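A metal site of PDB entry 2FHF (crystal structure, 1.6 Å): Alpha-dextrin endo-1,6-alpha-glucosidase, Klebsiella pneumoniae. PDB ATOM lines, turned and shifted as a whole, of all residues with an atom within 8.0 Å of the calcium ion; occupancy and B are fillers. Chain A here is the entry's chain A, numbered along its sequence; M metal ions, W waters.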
ATOM      1  N   THR A 484     -12.154 -21.229  29.958  1.00  0.00           N
ATOM      2  CA  THR A 484     -10.912 -20.581  29.538  1.00  0.00           C
ATOM      3  C   THR A 484     -10.144 -21.050  28.301  1.00  0.00           C
ATOM      4  O   THR A 484      -8.969 -20.717  28.133  1.00  0.00           O
ATOM      5  CB  THR A 484      -9.966 -20.510  30.740  1.00  0.00           C
ATOM      6  OG1 THR A 484      -9.928 -21.786  31.383  1.00  0.00           O
ATOM      7  CG2 THR A 484     -10.474 -19.466  31.732  1.00  0.00           C
ATOM      8  N   VAL A 485     -10.803 -21.826  27.445  1.00  0.00           N
ATOM      9  CA  VAL A 485     -10.219 -22.271  26.187  1.00  0.00           C
ATOM     10  C   VAL A 485     -11.310 -22.095  25.140  1.00  0.00           C
ATOM     11  O   VAL A 485     -12.436 -22.572  25.318  1.00  0.00           O
ATOM     12  CB  VAL A 485      -9.785 -23.756  26.228  1.00  0.00           C
ATOM     13  CG1 VAL A 485      -9.469 -24.250  24.827  1.00  0.00           C
ATOM     14  CG2 VAL A 485      -8.547 -23.903  27.113  1.00  0.00           C
ATOM     15  N   ASN A 486     -11.007 -21.384  24.062  1.00  0.00           N
ATOM     16  CA  ASN A 486     -12.007 -21.183  23.023  1.00  0.00           C
ATOM     17  C   ASN A 486     -12.142 -22.492  22.248  1.00  0.00           C
ATOM     18  O   ASN A 486     -11.160 -23.011  21.717  1.00  0.00           O
ATOM     19  CB  ASN A 486     -11.602 -20.043  22.082  1.00  0.00           C
ATOM     20  CG  ASN A 486     -12.760 -19.537  21.257  1.00  0.00           C
ATOM     21  OD1 ASN A 486     -13.553 -20.329  20.750  1.00  0.00           O
ATOM     22  ND2 ASN A 486     -12.871 -18.224  21.113  1.00  0.00           N
ATOM     23  N   ASP A 494      -1.772 -22.707  18.488  1.00  0.00           N
ATOM     24  CA  ASP A 494      -0.899 -23.429  19.399  1.00  0.00           C
ATOM     25  C   ASP A 494       0.555 -23.346  18.944  1.00  0.00           C
ATOM     26  O   ASP A 494       0.835 -23.009  17.798  1.00  0.00           O
ATOM     27  CB  ASP A 494      -1.385 -24.878  19.559  1.00  0.00           C
ATOM     28  CG  ASP A 494      -2.602 -24.974  20.477  1.00  0.00           C
ATOM     29  OD1 ASP A 494      -2.455 -24.631  21.680  1.00  0.00           O
ATOM     30  OD2 ASP A 494      -3.690 -25.379  20.016  1.00  0.00           O
ATOM     31  N   ASN A 546       5.590 -16.370  25.558  1.00  0.00           N
ATOM     32  CA  ASN A 546       4.627 -17.379  25.980  1.00  0.00           C
ATOM     33  C   ASN A 546       3.428 -16.789  26.712  1.00  0.00           C
ATOM     34  O   ASN A 546       2.330 -17.352  26.653  1.00  0.00           O
ATOM     35  CB  ASN A 546       5.297 -18.434  26.871  1.00  0.00           C
ATOM     36  CG  ASN A 546       4.519 -19.736  26.895  1.00  0.00           C
ATOM     37  OD1 ASN A 546       4.265 -20.329  25.851  1.00  0.00           O
ATOM     38  ND2 ASN A 546       4.129 -20.182  28.088  1.00  0.00           N
ATOM     39  N   THR A 547       3.632 -15.670  27.402  1.00  0.00           N
ATOM     40  CA  THR A 547       2.530 -15.035  28.129  1.00  0.00           C
ATOM     41  C   THR A 547       1.465 -14.559  27.153  1.00  0.00           C
ATOM     42  O   THR A 547       0.277 -14.568  27.466  1.00  0.00           O
ATOM     43  CB  THR A 547       3.043 -13.848  28.973  1.00  0.00           C
ATOM     44  OG1 THR A 547       3.879 -14.355  30.027  1.00  0.00           O
ATOM     45  CG2 THR A 547       1.877 -13.095  29.599  1.00  0.00           C
ATOM     46  N   LEU A 548       1.892 -14.139  25.969  1.00  0.00           N
ATOM     47  CA  LEU A 548       0.950 -13.672  24.947  1.00  0.00           C
ATOM     48  C   LEU A 548       0.282 -14.899  24.318  1.00  0.00           C
ATOM     49  O   LEU A 548      -0.934 -14.903  24.091  1.00  0.00           O
ATOM     50  CB  LEU A 548       1.694 -12.856  23.883  1.00  0.00           C
ATOM     51  CG  LEU A 548       2.394 -11.586  24.390  1.00  0.00           C
ATOM     52  CD1 LEU A 548       3.105 -10.891  23.233  1.00  0.00           C
ATOM     53  CD2 LEU A 548       1.382 -10.657  25.036  1.00  0.00           C
ATOM     54  N   VAL A 549       1.085 -15.931  24.039  1.00  0.00           N
ATOM     55  CA  VAL A 549       0.572 -17.165  23.440  1.00  0.00           C
ATOM     56  C   VAL A 549      -0.548 -17.777  24.285  1.00  0.00           C
ATOM     57  O   VAL A 549      -1.538 -18.275  23.759  1.00  0.00           O
ATOM     58  CB  VAL A 549       1.709 -18.208  23.309  1.00  0.00           C
ATOM     59  CG1 VAL A 549       1.137 -19.550  22.875  1.00  0.00           C
ATOM     60  CG2 VAL A 549       2.763 -17.726  22.305  1.00  0.00           C
ATOM     61  N   ALA A 550      -0.372 -17.725  25.598  1.00  0.00           N
ATOM     62  CA  ALA A 550      -1.341 -18.292  26.541  1.00  0.00           C
ATOM     63  C   ALA A 550      -2.769 -17.769  26.391  1.00  0.00           C
ATOM     64  O   ALA A 550      -3.735 -18.477  26.711  1.00  0.00           O
ATOM     65  CB  ALA A 550      -0.852 -18.064  27.968  1.00  0.00           C
ATOM     66  N   GLN A 551      -2.899 -16.528  25.926  1.00  0.00           N
ATOM     67  CA  GLN A 551      -4.196 -15.890  25.759  1.00  0.00           C
ATOM     68  C   GLN A 551      -5.085 -16.567  24.720  1.00  0.00           C
ATOM     69  O   GLN A 551      -6.317 -16.544  24.843  1.00  0.00           O
ATOM     70  CB  GLN A 551      -4.027 -14.419  25.357  1.00  0.00           C
ATOM     71  CG  GLN A 551      -3.250 -13.581  26.354  1.00  0.00           C
ATOM     72  CD  GLN A 551      -2.805 -12.252  25.758  1.00  0.00           C
ATOM     73  OE1 GLN A 551      -2.286 -11.392  26.464  1.00  0.00           O
ATOM     74  NE2 GLN A 551      -3.013 -12.079  24.461  1.00  0.00           N
ATOM     75  N   THR A 552      -4.477 -17.170  23.714  1.00  0.00           N
ATOM     76  CA  THR A 552      -5.232 -17.790  22.637  1.00  0.00           C
ATOM     77  C   THR A 552      -4.861 -19.230  22.280  1.00  0.00           C
ATOM     78  O   THR A 552      -5.148 -19.673  21.162  1.00  0.00           O
ATOM     79  CB  THR A 552      -5.155 -16.921  21.356  1.00  0.00           C
ATOM     80  OG1 THR A 552      -3.791 -16.594  21.086  1.00  0.00           O
ATOM     81  CG2 THR A 552      -5.945 -15.620  21.529  1.00  0.00           C
ATOM     82  N   ASP A 553      -4.242 -19.963  23.197  1.00  0.00           N
ATOM     83  CA  ASP A 553      -3.876 -21.342  22.911  1.00  0.00           C
ATOM     84  C   ASP A 553      -4.937 -22.313  23.431  1.00  0.00           C
ATOM     85  O   ASP A 553      -5.990 -21.886  23.911  1.00  0.00           O
ATOM     86  CB  ASP A 553      -2.488 -21.696  23.483  1.00  0.00           C
ATOM     87  CG  ASP A 553      -2.414 -21.600  24.998  1.00  0.00           C
ATOM     88  OD1 ASP A 553      -3.469 -21.470  25.668  1.00  0.00           O
ATOM     89  OD2 ASP A 553      -1.280 -21.656  25.537  1.00  0.00           O
ATOM     90  N   SER A 554      -4.675 -23.609  23.321  1.00  0.00           N
ATOM     91  CA  SER A 554      -5.618 -24.627  23.780  1.00  0.00           C
ATOM     92  C   SER A 554      -5.354 -25.048  25.215  1.00  0.00           C
ATOM     93  O   SER A 554      -5.968 -26.005  25.707  1.00  0.00           O
ATOM     94  CB  SER A 554      -5.510 -25.875  22.897  1.00  0.00           C
ATOM     95  OG  SER A 554      -5.840 -25.617  21.543  1.00  0.00           O
ATOM     96  N   TYR A 555      -4.466 -24.340  25.905  1.00  0.00           N
ATOM     97  CA  TYR A 555      -4.079 -24.740  27.245  1.00  0.00           C
ATOM     98  C   TYR A 555      -4.590 -23.990  28.479  1.00  0.00           C
ATOM     99  O   TYR A 555      -4.543 -22.760  28.560  1.00  0.00           O
ATOM    100  CB  TYR A 555      -2.550 -24.783  27.339  1.00  0.00           C
ATOM    101  CG  TYR A 555      -2.034 -25.549  28.543  1.00  0.00           C
ATOM    102  CD1 TYR A 555      -2.133 -25.028  29.830  1.00  0.00           C
ATOM    103  CD2 TYR A 555      -1.537 -26.841  28.397  1.00  0.00           C
ATOM    104  CE1 TYR A 555      -1.756 -25.780  30.940  1.00  0.00           C
ATOM    105  CE2 TYR A 555      -1.144 -27.601  29.502  1.00  0.00           C
ATOM    106  CZ  TYR A 555      -1.271 -27.066  30.764  1.00  0.00           C
ATOM    107  OH  TYR A 555      -0.941 -27.843  31.851  1.00  0.00           O
ATOM    108  N   ASN A 556      -5.069 -24.772  29.443  1.00  0.00           N
ATOM    109  CA  ASN A 556      -5.494 -24.263  30.751  1.00  0.00           C
ATOM    110  C   ASN A 556      -5.852 -25.446  31.632  1.00  0.00           C
ATOM    111  O   ASN A 556      -6.439 -26.422  31.161  1.00  0.00           O
ATOM    112  CB  ASN A 556      -6.696 -23.306  30.652  1.00  0.00           C
ATOM    113  CG  ASN A 556      -6.838 -22.429  31.895  1.00  0.00           C
ATOM    114  OD1 ASN A 556      -7.145 -22.905  32.995  1.00  0.00           O
ATOM    115  ND2 ASN A 556      -6.593 -21.126  31.732  1.00  0.00           N
ATOM    116  N   TRP A 557      -5.469 -25.375  32.901  1.00  0.00           N
ATOM    117  CA  TRP A 557      -5.813 -26.452  33.823  1.00  0.00           C
ATOM    118  C   TRP A 557      -7.335 -26.609  33.805  1.00  0.00           C
ATOM    119  O   TRP A 557      -7.857 -27.713  33.939  1.00  0.00           O
ATOM    120  CB  TRP A 557      -5.392 -26.117  35.242  1.00  0.00           C
ATOM    121  CG  TRP A 557      -3.948 -26.326  35.514  1.00  0.00           C
ATOM    122  CD1 TRP A 557      -3.041 -27.004  34.740  1.00  0.00           C
ATOM    123  CD2 TRP A 557      -3.223 -25.870  36.662  1.00  0.00           C
ATOM    124  NE1 TRP A 557      -1.806 -26.999  35.344  1.00  0.00           N
ATOM    125  CE2 TRP A 557      -1.894 -26.311  36.519  1.00  0.00           C
ATOM    126  CE3 TRP A 557      -3.581 -25.131  37.798  1.00  0.00           C
ATOM    127  CZ2 TRP A 557      -0.905 -26.023  37.473  1.00  0.00           C
ATOM    128  CZ3 TRP A 557      -2.606 -24.852  38.747  1.00  0.00           C
ATOM    129  CH2 TRP A 557      -1.282 -25.299  38.575  1.00  0.00           C
ATOM    130  N   TYR A 892      -0.898 -22.981  35.643  1.00  0.00           N
ATOM    131  CA  TYR A 892      -2.249 -23.125  35.076  1.00  0.00           C
ATOM    132  C   TYR A 892      -2.484 -22.591  33.671  1.00  0.00           C
ATOM    133  O   TYR A 892      -3.307 -23.134  32.935  1.00  0.00           O
ATOM    134  CB  TYR A 892      -3.302 -22.500  36.015  1.00  0.00           C
ATOM    135  CG  TYR A 892      -3.402 -21.000  35.912  1.00  0.00           C
ATOM    136  CD1 TYR A 892      -2.405 -20.171  36.421  1.00  0.00           C
ATOM    137  CD2 TYR A 892      -4.509 -20.403  35.305  1.00  0.00           C
ATOM    138  CE1 TYR A 892      -2.500 -18.777  36.319  1.00  0.00           C
ATOM    139  CE2 TYR A 892      -4.611 -19.005  35.196  1.00  0.00           C
ATOM    140  CZ  TYR A 892      -3.599 -18.200  35.707  1.00  0.00           C
ATOM    141  OH  TYR A 892      -3.701 -16.834  35.629  1.00  0.00           O
ATOM    142  N   ASP A 893      -1.788 -21.521  33.309  1.00  0.00           N
ATOM    143  CA  ASP A 893      -1.953 -20.901  32.001  1.00  0.00           C
ATOM    144  C   ASP A 893      -0.580 -20.742  31.341  1.00  0.00           C
ATOM    145  O   ASP A 893      -0.392 -19.878  30.476  1.00  0.00           O
ATOM    146  CB  ASP A 893      -2.605 -19.520  32.176  1.00  0.00           C
ATOM    147  CG  ASP A 893      -3.241 -18.996  30.893  1.00  0.00           C
ATOM    148  OD1 ASP A 893      -3.607 -17.794  30.876  1.00  0.00           O
ATOM    149  OD2 ASP A 893      -3.392 -19.761  29.926  1.00  0.00           O
ATOM    150  N   SER A 894       0.364 -21.588  31.741  1.00  0.00           N
ATOM    151  CA  SER A 894       1.722 -21.514  31.195  1.00  0.00           C
ATOM    152  C   SER A 894       1.954 -22.327  29.935  1.00  0.00           C
ATOM    153  O   SER A 894       3.086 -22.507  29.486  1.00  0.00           O
ATOM    154  CB  SER A 894       2.743 -21.892  32.274  1.00  0.00           C
ATOM    155  OG  SER A 894       2.846 -20.856  33.235  1.00  0.00           O
ATOM    156  N   GLY A 895       0.853 -22.832  29.370  1.00  0.00           N
ATOM    157  CA  GLY A 895       0.911 -23.578  28.116  1.00  0.00           C
ATOM    158  C   GLY A 895       1.650 -24.891  27.993  1.00  0.00           C
ATOM    159  O   GLY A 895       2.124 -25.475  28.977  1.00  0.00           O
ATOM    160  N   ASP A 896       1.731 -25.377  26.761  1.00  0.00           N
ATOM    161  CA  ASP A 896       2.416 -26.620  26.465  1.00  0.00           C
ATOM    162  C   ASP A 896       3.915 -26.521  26.781  1.00  0.00           C
ATOM    163  O   ASP A 896       4.546 -27.500  27.150  1.00  0.00           O
ATOM    164  CB  ASP A 896       2.290 -26.991  24.986  1.00  0.00           C
ATOM    165  CG  ASP A 896       0.888 -27.398  24.570  1.00  0.00           C
ATOM    166  OD1 ASP A 896       0.085 -27.823  25.436  1.00  0.00           O
ATOM    167  OD2 ASP A 896       0.580 -27.315  23.365  1.00  0.00           O
HETATM  168 CA    CA M   1      -4.223 -20.550  27.790  1.00  0.00          CA
HETATM  169  O   HOH W   1      -1.746 -21.208  28.068  1.00  0.00           O
HETATM  170  O   HOH W   2      -6.307 -19.985  29.062  1.00  0.00           O
HETATM  171  O   HOH W   3      -6.063 -20.673  26.361  1.00  0.00           O
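The nearest printed residue that does not touch the calcium ion is Asn 556 (4.6 Å).
Water W3 is bound to the calcium ion (2.3 Å). O of Tyr 555 is bound to the calcium ion, 2.4 Å away. The backbone carbonyl oxygen (O) of Ala 550 is bound to the calcium ion. The calcium ion is bound by the side-chain carboxylate (OD2) of Asp 893 (2.4 Å). The calcium ion is bound by the side-chain carboxylate (OD1) of Asp 553, at 2.4 Å. Water W2 binds the calcium ion. Water W1 is bound to the calcium ion (2.6 Å).
Water W2 lies within hydrogen-bond range of the backbone carbonyl oxygen of Thr 484 and the side-chain amide nitrogen of Asn 556. Water W3 lies within hydrogen-bond range of O of Asp 553 (2.7 Å) and O of Thr 484 (3.4 Å). Water W1 lies within hydrogen-bond range of OD2 of Asp 553 (2.6 Å), O of Asp 893 (3.1 Å) and N of Gly 895 (3.3 Å).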
